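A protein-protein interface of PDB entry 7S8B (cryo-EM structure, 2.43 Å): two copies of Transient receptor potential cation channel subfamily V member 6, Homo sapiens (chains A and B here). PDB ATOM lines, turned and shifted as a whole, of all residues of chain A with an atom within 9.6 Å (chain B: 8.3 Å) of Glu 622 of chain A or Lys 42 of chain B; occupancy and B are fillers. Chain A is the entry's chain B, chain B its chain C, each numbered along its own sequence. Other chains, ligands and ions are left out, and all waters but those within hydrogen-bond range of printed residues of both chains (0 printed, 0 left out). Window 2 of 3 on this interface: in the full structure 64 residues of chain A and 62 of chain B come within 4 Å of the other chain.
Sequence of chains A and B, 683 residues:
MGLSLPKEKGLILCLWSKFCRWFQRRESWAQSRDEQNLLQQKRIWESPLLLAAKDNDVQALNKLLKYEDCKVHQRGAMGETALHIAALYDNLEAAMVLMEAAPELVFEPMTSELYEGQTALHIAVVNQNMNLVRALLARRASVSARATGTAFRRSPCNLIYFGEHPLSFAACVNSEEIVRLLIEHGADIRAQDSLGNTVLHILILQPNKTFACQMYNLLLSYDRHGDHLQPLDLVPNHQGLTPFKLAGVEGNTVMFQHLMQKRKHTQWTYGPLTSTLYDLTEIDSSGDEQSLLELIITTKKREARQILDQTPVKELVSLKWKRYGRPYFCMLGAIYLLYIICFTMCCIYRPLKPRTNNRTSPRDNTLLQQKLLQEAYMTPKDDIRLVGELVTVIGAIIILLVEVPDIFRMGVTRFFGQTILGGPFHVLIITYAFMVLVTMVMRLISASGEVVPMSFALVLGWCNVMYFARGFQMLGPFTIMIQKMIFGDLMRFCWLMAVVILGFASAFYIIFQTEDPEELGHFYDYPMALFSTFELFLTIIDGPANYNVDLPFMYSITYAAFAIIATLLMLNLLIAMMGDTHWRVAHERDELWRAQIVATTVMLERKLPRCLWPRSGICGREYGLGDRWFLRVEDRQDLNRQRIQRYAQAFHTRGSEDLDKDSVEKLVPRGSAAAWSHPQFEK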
ATOM      1  N   HIS A 265      36.391  25.081  -7.359  1.00  0.00           N
ATOM      2  CA  HIS A 265      35.512  24.570  -8.405  1.00  0.00           C
ATOM      3  C   HIS A 265      34.959  25.759  -9.169  1.00  0.00           C
ATOM      4  O   HIS A 265      34.310  26.622  -8.576  1.00  0.00           O
ATOM      5  CB  HIS A 265      34.375  23.728  -7.837  1.00  0.00           C
ATOM      6  CG  HIS A 265      33.443  23.217  -8.883  1.00  0.00           C
ATOM      7  ND1 HIS A 265      33.731  22.120  -9.666  1.00  0.00           N
ATOM      8  CD2 HIS A 265      32.258  23.695  -9.328  1.00  0.00           C
ATOM      9  CE1 HIS A 265      32.745  21.919 -10.519  1.00  0.00           C
ATOM     10  NE2 HIS A 265      31.839  22.862 -10.337  1.00  0.00           N
ATOM     11  N   GLN A 267      32.426  27.494 -11.311  1.00  0.00           N
ATOM     12  CA  GLN A 267      31.014  27.312 -11.636  1.00  0.00           C
ATOM     13  C   GLN A 267      30.717  27.702 -13.076  1.00  0.00           C
ATOM     14  O   GLN A 267      30.079  26.946 -13.815  1.00  0.00           O
ATOM     15  CB  GLN A 267      30.148  28.136 -10.691  1.00  0.00           C
ATOM     16  CG  GLN A 267      30.139  27.654  -9.269  1.00  0.00           C
ATOM     17  CD  GLN A 267      29.234  28.483  -8.400  1.00  0.00           C
ATOM     18  OE1 GLN A 267      28.684  29.486  -8.840  1.00  0.00           O
ATOM     19  NE2 GLN A 267      29.059  28.061  -7.166  1.00  0.00           N
ATOM     20  N   ILE A 618      28.268  28.531   2.457  1.00  0.00           N
ATOM     21  CA  ILE A 618      26.981  27.943   2.107  1.00  0.00           C
ATOM     22  C   ILE A 618      27.135  26.443   2.225  1.00  0.00           C
ATOM     23  O   ILE A 618      28.027  25.860   1.602  1.00  0.00           O
ATOM     24  CB  ILE A 618      26.546  28.325   0.687  1.00  0.00           C
ATOM     25  CG1 ILE A 618      26.457  29.832   0.553  1.00  0.00           C
ATOM     26  CG2 ILE A 618      25.200  27.707   0.356  1.00  0.00           C
ATOM     27  CD1 ILE A 618      26.325  30.272  -0.853  1.00  0.00           C
ATOM     28  N   CYS A 619      26.284  25.819   3.026  1.00  0.00           N
ATOM     29  CA  CYS A 619      26.346  24.382   3.197  1.00  0.00           C
ATOM     30  C   CYS A 619      25.739  23.692   1.989  1.00  0.00           C
ATOM     31  O   CYS A 619      24.762  24.171   1.407  1.00  0.00           O
ATOM     32  CB  CYS A 619      25.609  23.964   4.469  1.00  0.00           C
ATOM     33  SG  CYS A 619      25.612  22.207   4.832  1.00  0.00           S
ATOM     34  N   GLY A 620      26.303  22.544   1.634  1.00  0.00           N
ATOM     35  CA  GLY A 620      25.717  21.676   0.632  1.00  0.00           C
ATOM     36  C   GLY A 620      24.504  20.932   1.154  1.00  0.00           C
ATOM     37  O   GLY A 620      23.744  21.438   1.985  1.00  0.00           O
ATOM     38  N   ARG A 621      24.273  19.744   0.579  1.00  0.00           N
ATOM     39  CA  ARG A 621      23.192  18.782   0.852  1.00  0.00           C
ATOM     40  C   ARG A 621      21.835  19.282   0.345  1.00  0.00           C
ATOM     41  O   ARG A 621      20.902  18.491   0.180  1.00  0.00           O
ATOM     42  CB  ARG A 621      23.139  18.411   2.354  1.00  0.00           C
ATOM     43  CG  ARG A 621      22.324  17.171   2.762  1.00  0.00           C
ATOM     44  CD  ARG A 621      20.910  17.502   3.235  1.00  0.00           C
ATOM     45  NE  ARG A 621      20.889  18.397   4.387  1.00  0.00           N
ATOM     46  CZ  ARG A 621      19.813  19.070   4.786  1.00  0.00           C
ATOM     47  NH1 ARG A 621      18.668  18.944   4.126  1.00  0.00           N
ATOM     48  NH2 ARG A 621      19.875  19.863   5.844  1.00  0.00           N
ATOM     49  N   GLU A 622      21.739  20.562  -0.009  1.00  0.00           N
ATOM     50  CA  GLU A 622      20.662  21.092  -0.826  1.00  0.00           C
ATOM     51  C   GLU A 622      21.156  21.479  -2.207  1.00  0.00           C
ATOM     52  O   GLU A 622      20.413  22.106  -2.967  1.00  0.00           O
ATOM     53  CB  GLU A 622      20.006  22.310  -0.167  1.00  0.00           C
ATOM     54  CG  GLU A 622      19.132  22.033   1.038  1.00  0.00           C
ATOM     55  CD  GLU A 622      19.874  22.098   2.348  1.00  0.00           C
ATOM     56  OE1 GLU A 622      21.087  22.399   2.347  1.00  0.00           O
ATOM     57  OE2 GLU A 622      19.237  21.868   3.396  1.00  0.00           O
ATOM     58  N   TYR A 623      22.403  21.153  -2.537  1.00  0.00           N
ATOM     59  CA  TYR A 623      22.957  21.499  -3.837  1.00  0.00           C
ATOM     60  C   TYR A 623      23.785  20.365  -4.426  1.00  0.00           C
ATOM     61  O   TYR A 623      24.484  20.583  -5.423  1.00  0.00           O
ATOM     62  CB  TYR A 623      23.810  22.769  -3.753  1.00  0.00           C
ATOM     63  CG  TYR A 623      23.044  23.985  -3.296  1.00  0.00           C
ATOM     64  CD1 TYR A 623      22.087  24.570  -4.109  1.00  0.00           C
ATOM     65  CD2 TYR A 623      23.300  24.569  -2.067  1.00  0.00           C
ATOM     66  CE1 TYR A 623      21.383  25.679  -3.693  1.00  0.00           C
ATOM     67  CE2 TYR A 623      22.608  25.679  -1.648  1.00  0.00           C
ATOM     68  CZ  TYR A 623      21.651  26.232  -2.465  1.00  0.00           C
ATOM     69  OH  TYR A 623      20.953  27.344  -2.056  1.00  0.00           O
ATOM     70  N   GLY A 624      23.733  19.170  -3.849  1.00  0.00           N
ATOM     71  CA  GLY A 624      24.503  18.061  -4.374  1.00  0.00           C
ATOM     72  C   GLY A 624      25.988  18.185  -4.151  1.00  0.00           C
ATOM     73  O   GLY A 624      26.774  17.673  -4.955  1.00  0.00           O
ATOM     74  N   LEU A 625      26.398  18.860  -3.083  1.00  0.00           N
ATOM     75  CA  LEU A 625      27.800  19.159  -2.858  1.00  0.00           C
ATOM     76  C   LEU A 625      28.381  18.468  -1.631  1.00  0.00           C
ATOM     77  O   LEU A 625      29.591  18.560  -1.407  1.00  0.00           O
ATOM     78  CB  LEU A 625      27.984  20.676  -2.743  1.00  0.00           C
ATOM     79  CG  LEU A 625      27.630  21.507  -3.985  1.00  0.00           C
ATOM     80  CD1 LEU A 625      27.650  22.988  -3.651  1.00  0.00           C
ATOM     81  CD2 LEU A 625      28.575  21.215  -5.147  1.00  0.00           C
ATOM     82  N   GLY A 626      27.567  17.772  -0.849  1.00  0.00           N
ATOM     83  CA  GLY A 626      28.028  17.107   0.351  1.00  0.00           C
ATOM     84  C   GLY A 626      27.602  17.822   1.617  1.00  0.00           C
ATOM     85  O   GLY A 626      26.740  18.701   1.618  1.00  0.00           O
ATOM     86  N   ASP A 627      28.231  17.424   2.725  1.00  0.00           N
ATOM     87  CA  ASP A 627      28.039  18.086   4.011  1.00  0.00           C
ATOM     88  C   ASP A 627      29.047  19.202   4.241  1.00  0.00           C
ATOM     89  O   ASP A 627      29.333  19.552   5.394  1.00  0.00           O
ATOM     90  CB  ASP A 627      28.108  17.062   5.145  1.00  0.00           C
ATOM     91  CG  ASP A 627      26.958  16.075   5.106  1.00  0.00           C
ATOM     92  OD1 ASP A 627      25.878  16.437   4.604  1.00  0.00           O
ATOM     93  OD2 ASP A 627      27.133  14.938   5.590  1.00  0.00           O
ATOM     94  N   ARG A 628      29.594  19.761   3.170  1.00  0.00           N
ATOM     95  CA  ARG A 628      30.620  20.785   3.213  1.00  0.00           C
ATOM     96  C   ARG A 628      29.996  22.172   3.136  1.00  0.00           C
ATOM     97  O   ARG A 628      28.906  22.359   2.600  1.00  0.00           O
ATOM     98  CB  ARG A 628      31.594  20.589   2.053  1.00  0.00           C
ATOM     99  CG  ARG A 628      32.354  19.288   2.103  1.00  0.00           C
ATOM    100  CD  ARG A 628      33.193  19.104   0.863  1.00  0.00           C
ATOM    101  NE  ARG A 628      33.983  17.882   0.913  1.00  0.00           N
ATOM    102  CZ  ARG A 628      35.182  17.798   1.479  1.00  0.00           C
ATOM    103  NH1 ARG A 628      35.840  16.649   1.481  1.00  0.00           N
ATOM    104  NH2 ARG A 628      35.726  18.864   2.045  1.00  0.00           N
ATOM    105  N   TRP A 629      30.715  23.146   3.675  1.00  0.00           N
ATOM    106  CA  TRP A 629      30.359  24.554   3.604  1.00  0.00           C
ATOM    107  C   TRP A 629      31.284  25.225   2.602  1.00  0.00           C
ATOM    108  O   TRP A 629      32.501  25.117   2.730  1.00  0.00           O
ATOM    109  CB  TRP A 629      30.503  25.207   4.976  1.00  0.00           C
ATOM    110  CG  TRP A 629      29.495  24.744   5.954  1.00  0.00           C
ATOM    111  CD1 TRP A 629      29.565  23.633   6.734  1.00  0.00           C
ATOM    112  CD2 TRP A 629      28.283  25.406   6.312  1.00  0.00           C
ATOM    113  NE1 TRP A 629      28.460  23.540   7.531  1.00  0.00           N
ATOM    114  CE2 TRP A 629      27.657  24.622   7.291  1.00  0.00           C
ATOM    115  CE3 TRP A 629      27.660  26.579   5.890  1.00  0.00           C
ATOM    116  CZ2 TRP A 629      26.440  24.977   7.859  1.00  0.00           C
ATOM    117  CZ3 TRP A 629      26.459  26.922   6.441  1.00  0.00           C
ATOM    118  CH2 TRP A 629      25.855  26.126   7.415  1.00  0.00           C
ATOM    119  N   PHE A 630      30.713  25.933   1.631  1.00  0.00           N
ATOM    120  CA  PHE A 630      31.444  26.470   0.490  1.00  0.00           C
ATOM    121  C   PHE A 630      31.403  27.993   0.457  1.00  0.00           C
ATOM    122  O   PHE A 630      30.388  28.604   0.785  1.00  0.00           O
ATOM    123  CB  PHE A 630      30.853  25.952  -0.818  1.00  0.00           C
ATOM    124  CG  PHE A 630      31.174  24.527  -1.122  1.00  0.00           C
ATOM    125  CD1 PHE A 630      32.311  24.195  -1.830  1.00  0.00           C
ATOM    126  CD2 PHE A 630      30.337  23.517  -0.695  1.00  0.00           C
ATOM    127  CE1 PHE A 630      32.602  22.888  -2.117  1.00  0.00           C
ATOM    128  CE2 PHE A 630      30.628  22.216  -0.973  1.00  0.00           C
ATOM    129  CZ  PHE A 630      31.760  21.896  -1.687  1.00  0.00           C
ATOM    130  N   GLU B  35      23.239  32.131  -3.447  1.00  0.00           N
ATOM    131  CA  GLU B  35      22.430  30.917  -3.495  1.00  0.00           C
ATOM    132  C   GLU B  35      21.889  30.618  -4.884  1.00  0.00           C
ATOM    133  O   GLU B  35      21.686  29.450  -5.219  1.00  0.00           O
ATOM    134  CB  GLU B  35      21.261  31.001  -2.518  1.00  0.00           C
ATOM    135  CG  GLU B  35      21.595  30.674  -1.085  1.00  0.00           C
ATOM    136  CD  GLU B  35      20.391  30.840  -0.180  1.00  0.00           C
ATOM    137  OE1 GLU B  35      19.389  31.432  -0.637  1.00  0.00           O
ATOM    138  OE2 GLU B  35      20.433  30.362   0.974  1.00  0.00           O
ATOM    139  N   GLN B  36      21.631  31.647  -5.690  1.00  0.00           N
ATOM    140  CA  GLN B  36      21.061  31.428  -7.011  1.00  0.00           C
ATOM    141  C   GLN B  36      22.072  30.834  -7.975  1.00  0.00           C
ATOM    142  O   GLN B  36      21.695  30.060  -8.862  1.00  0.00           O
ATOM    143  CB  GLN B  36      20.488  32.736  -7.545  1.00  0.00           C
ATOM    144  CG  GLN B  36      19.210  33.122  -6.829  1.00  0.00           C
ATOM    145  CD  GLN B  36      18.726  34.512  -7.163  1.00  0.00           C
ATOM    146  OE1 GLN B  36      19.394  35.268  -7.867  1.00  0.00           O
ATOM    147  NE2 GLN B  36      17.550  34.860  -6.656  1.00  0.00           N
ATOM    148  N   ASN B  37      23.354  31.162  -7.810  1.00  0.00           N
ATOM    149  CA  ASN B  37      24.375  30.538  -8.634  1.00  0.00           C
ATOM    150  C   ASN B  37      24.576  29.076  -8.269  1.00  0.00           C
ATOM    151  O   ASN B  37      24.883  28.263  -9.145  1.00  0.00           O
ATOM    152  CB  ASN B  37      25.691  31.304  -8.524  1.00  0.00           C
ATOM    153  CG  ASN B  37      25.619  32.667  -9.163  1.00  0.00           C
ATOM    154  OD1 ASN B  37      25.803  33.686  -8.509  1.00  0.00           O
ATOM    155  ND2 ASN B  37      25.332  32.692 -10.453  1.00  0.00           N
ATOM    156  N   LEU B  38      24.381  28.714  -7.001  1.00  0.00           N
ATOM    157  CA  LEU B  38      24.454  27.311  -6.617  1.00  0.00           C
ATOM    158  C   LEU B  38      23.181  26.562  -6.954  1.00  0.00           C
ATOM    159  O   LEU B  38      23.249  25.399  -7.363  1.00  0.00           O
ATOM    160  CB  LEU B  38      24.751  27.160  -5.120  1.00  0.00           C
ATOM    161  CG  LEU B  38      26.209  27.157  -4.640  1.00  0.00           C
ATOM    162  CD1 LEU B  38      26.841  28.508  -4.707  1.00  0.00           C
ATOM    163  CD2 LEU B  38      26.290  26.643  -3.216  1.00  0.00           C
ATOM    164  N   LEU B  39      22.025  27.210  -6.814  1.00  0.00           N
ATOM    165  CA  LEU B  39      20.764  26.622  -7.245  1.00  0.00           C
ATOM    166  C   LEU B  39      20.692  26.469  -8.756  1.00  0.00           C
ATOM    167  O   LEU B  39      19.945  25.619  -9.240  1.00  0.00           O
ATOM    168  CB  LEU B  39      19.601  27.482  -6.748  1.00  0.00           C
ATOM    169  CG  LEU B  39      18.128  27.136  -6.950  1.00  0.00           C
ATOM    170  CD1 LEU B  39      17.730  25.892  -6.178  1.00  0.00           C
ATOM    171  CD2 LEU B  39      17.284  28.325  -6.542  1.00  0.00           C
ATOM    172  N   GLN B  40      21.458  27.261  -9.512  1.00  0.00           N
ATOM    173  CA  GLN B  40      21.521  27.071 -10.958  1.00  0.00           C
ATOM    174  C   GLN B  40      22.255  25.787 -11.307  1.00  0.00           C
ATOM    175  O   GLN B  40      21.858  25.067 -12.231  1.00  0.00           O
ATOM    176  CB  GLN B  40      22.206  28.266 -11.625  1.00  0.00           C
ATOM    177  CG  GLN B  40      22.268  28.147 -13.147  1.00  0.00           C
ATOM    178  CD  GLN B  40      22.955  29.303 -13.820  1.00  0.00           C
ATOM    179  OE1 GLN B  40      23.352  30.270 -13.177  1.00  0.00           O
ATOM    180  NE2 GLN B  40      23.137  29.192 -15.128  1.00  0.00           N
ATOM    181  N   GLN B  41      23.314  25.470 -10.561  1.00  0.00           N
ATOM    182  CA  GLN B  41      24.108  24.277 -10.813  1.00  0.00           C
ATOM    183  C   GLN B  41      23.401  22.992 -10.410  1.00  0.00           C
ATOM    184  O   GLN B  41      23.837  21.913 -10.824  1.00  0.00           O
ATOM    185  CB  GLN B  41      25.438  24.372 -10.068  1.00  0.00           C
ATOM    186  CG  GLN B  41      26.288  25.538 -10.508  1.00  0.00           C
ATOM    187  CD  GLN B  41      26.786  25.376 -11.919  1.00  0.00           C
ATOM    188  OE1 GLN B  41      27.200  24.289 -12.316  1.00  0.00           O
ATOM    189  NE2 GLN B  41      26.743  26.452 -12.690  1.00  0.00           N
ATOM    190  N   LYS B  42      22.341  23.072  -9.610  1.00  0.00           N
ATOM    191  CA  LYS B  42      21.559  21.891  -9.279  1.00  0.00           C
ATOM    192  C   LYS B  42      20.408  21.666 -10.250  1.00  0.00           C
ATOM    193  O   LYS B  42      20.086  20.510 -10.554  1.00  0.00           O
ATOM    194  CB  LYS B  42      21.028  21.999  -7.845  1.00  0.00           C
ATOM    195  CG  LYS B  42      20.319  20.756  -7.353  1.00  0.00           C
ATOM    196  CD  LYS B  42      19.891  20.876  -5.916  1.00  0.00           C
ATOM    197  CE  LYS B  42      19.021  19.700  -5.511  1.00  0.00           C
ATOM    198  NZ  LYS B  42      19.772  18.415  -5.566  1.00  0.00           N
ATOM    199  N   ARG B  43      19.820  22.736 -10.804  1.00  0.00           N
ATOM    200  CA  ARG B  43      18.688  22.595 -11.720  1.00  0.00           C
ATOM    201  C   ARG B  43      19.071  22.027 -13.082  1.00  0.00           C
ATOM    202  O   ARG B  43      18.187  21.850 -13.925  1.00  0.00           O
ATOM    203  CB  ARG B  43      17.981  23.932 -11.937  1.00  0.00           C
ATOM    204  CG  ARG B  43      17.314  24.517 -10.707  1.00  0.00           C
ATOM    205  CD  ARG B  43      16.184  23.660 -10.200  1.00  0.00           C
ATOM    206  NE  ARG B  43      15.539  24.274  -9.045  1.00  0.00           N
ATOM    207  CZ  ARG B  43      14.589  23.688  -8.327  1.00  0.00           C
ATOM    208  NH1 ARG B  43      14.054  24.317  -7.292  1.00  0.00           N
ATOM    209  NH2 ARG B  43      14.178  22.467  -8.643  1.00  0.00           N
ATOM    210  N   ILE B  44      20.355  21.773 -13.334  1.00  0.00           N
ATOM    211  CA  ILE B  44      20.758  21.088 -14.552  1.00  0.00           C
ATOM    212  C   ILE B  44      20.601  19.577 -14.401  1.00  0.00           C
ATOM    213  O   ILE B  44      20.100  18.892 -15.302  1.00  0.00           O
ATOM    214  CB  ILE B  44      22.202  21.485 -14.907  1.00  0.00           C
ATOM    215  CG1 ILE B  44      22.277  22.980 -15.218  1.00  0.00           C
ATOM    216  CG2 ILE B  44      22.730  20.673 -16.073  1.00  0.00           C
ATOM    217  CD1 ILE B  44      23.682  23.493 -15.394  1.00  0.00           C
ATOM    218  N   TRP B  45      20.966  19.046 -13.234  1.00  0.00           N
ATOM    219  CA  TRP B  45      21.263  17.630 -13.068  1.00  0.00           C
ATOM    220  C   TRP B  45      20.041  16.723 -13.035  1.00  0.00           C
ATOM    221  O   TRP B  45      20.209  15.503 -13.134  1.00  0.00           O
ATOM    222  CB  TRP B  45      22.062  17.436 -11.787  1.00  0.00           C
ATOM    223  CG  TRP B  45      23.422  18.005 -11.872  1.00  0.00           C
ATOM    224  CD1 TRP B  45      24.077  18.396 -12.999  1.00  0.00           C
ATOM    225  CD2 TRP B  45      24.297  18.290 -10.780  1.00  0.00           C
ATOM    226  NE1 TRP B  45      25.314  18.887 -12.684  1.00  0.00           N
ATOM    227  CE2 TRP B  45      25.477  18.833 -11.326  1.00  0.00           C
ATOM    228  CE3 TRP B  45      24.203  18.129  -9.396  1.00  0.00           C
ATOM    229  CZ2 TRP B  45      26.551  19.220 -10.537  1.00  0.00           C
ATOM    230  CZ3 TRP B  45      25.274  18.512  -8.612  1.00  0.00           C
ATOM    231  CH2 TRP B  45      26.434  19.053  -9.185  1.00  0.00           C
ATOM    232  N   GLU B  46      18.826  17.250 -12.910  1.00  0.00           N
ATOM    233  CA  GLU B  46      17.669  16.380 -12.747  1.00  0.00           C
ATOM    234  C   GLU B  46      16.878  16.160 -14.036  1.00  0.00           C
ATOM    235  O   GLU B  46      15.754  15.654 -13.973  1.00  0.00           O
ATOM    236  CB  GLU B  46      16.742  16.914 -11.652  1.00  0.00           C
ATOM    237  CG  GLU B  46      16.060  18.242 -11.956  1.00  0.00           C
ATOM    238  CD  GLU B  46      15.087  18.639 -10.862  1.00  0.00           C
ATOM    239  OE1 GLU B  46      14.954  17.875  -9.881  1.00  0.00           O
ATOM    240  OE2 GLU B  46      14.452  19.707 -10.985  1.00  0.00           O
ATOM    241  N   SER B  47      17.432  16.507 -15.201  1.00  0.00           N
ATOM    242  CA  SER B  47      16.718  16.280 -16.454  1.00  0.00           C
ATOM    243  C   SER B  47      17.671  15.899 -17.579  1.00  0.00           C
ATOM    244  O   SER B  47      18.820  16.361 -17.600  1.00  0.00           O
ATOM    245  CB  SER B  47      15.909  17.517 -16.864  1.00  0.00           C
ATOM    246  OG  SER B  47      14.841  17.749 -15.961  1.00  0.00           O
ATOM    247  N   GLY B  76      15.212  26.457 -16.663  1.00  0.00           N
ATOM    248  CA  GLY B  76      16.156  26.289 -15.575  1.00  0.00           C
ATOM    249  C   GLY B  76      15.858  27.196 -14.401  1.00  0.00           C
ATOM    250  O   GLY B  76      14.704  27.540 -14.126  1.00  0.00           O
ATOM    251  N   ALA B  77      16.920  27.596 -13.698  1.00  0.00           N
ATOM    252  CA  ALA B  77      16.766  28.376 -12.473  1.00  0.00           C
ATOM    253  C   ALA B  77      16.411  29.825 -12.770  1.00  0.00           C
ATOM    254  O   ALA B  77      15.581  30.424 -12.077  1.00  0.00           O
ATOM    255  CB  ALA B  77      18.041  28.311 -11.637  1.00  0.00           C
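Of the printed residues of chain B, Ile 618 of chain A touches Leu 38. Of the printed residues of chain B, Tyr 623 of chain A touches Glu 35, Leu 38, Leu 39, Lys 42 and Trp 45. Of the printed residues of chain A, Asn 37 of chain B touches Gln 267 (3.5 Å). Of the printed residues of chain A, Leu 39 of chain B touches Tyr 623 (3.5 Å). Of chain A, only Glu 622 and Tyr 623 come within 4 Å of Lys 42 of chain B. Printed residues of chain A within 4 Å of Trp 45 of chain B: Tyr 623.
The backbone carbonyl oxygen of Ile 618 of chain A sits at hydrogen-bond distance from the backbone NH of Phe 630 of chain A, 2.7 Å away. The guanidinium group (NH1) of Arg 621 of chain A is in salt-bridge range of the side-chain carboxylate (OE2) of Glu 622 of chain A, 3.1 Å away.
No position is printed for both chains. Of the 11 pairs that touch across the chains among the printed residues, none has its exchanged pair printed and touching as well.
Among the printed residues, merely in contact across the chains: Gln 267 of chain A with Asn 37 of chain B, Gln 267 of chain A with Leu 38 of chain B, Gln 267 of chain A with Gln 41 of chain B, Ile 618 of chain A with Leu 38 of chain B, Glu 622 of chain A with Lys 42 of chain B, Tyr 623 of chain A with Glu 35 of chain B, Tyr 623 of chain A with Leu 38 of chain B, Tyr 623 of chain A with Leu 39 of chain B, Tyr 623 of chain A with Lys 42 of chain B, Tyr 623 of chain A with Trp 45 of chain B and Leu 625 of chain A with Leu 38 of chain B.
Along chain A the printed residues that touch a printed residue of chain B span positions 267 to 625. Hydrophobic or aromatic side chains of chain B that line the printed part of chain A: Leu 38, Leu 39 and Trp 45. Among the printed residues, no Asp or Glu carboxylate lies within 4 Å of a Lys or Arg side-chain nitrogen of the other chain.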
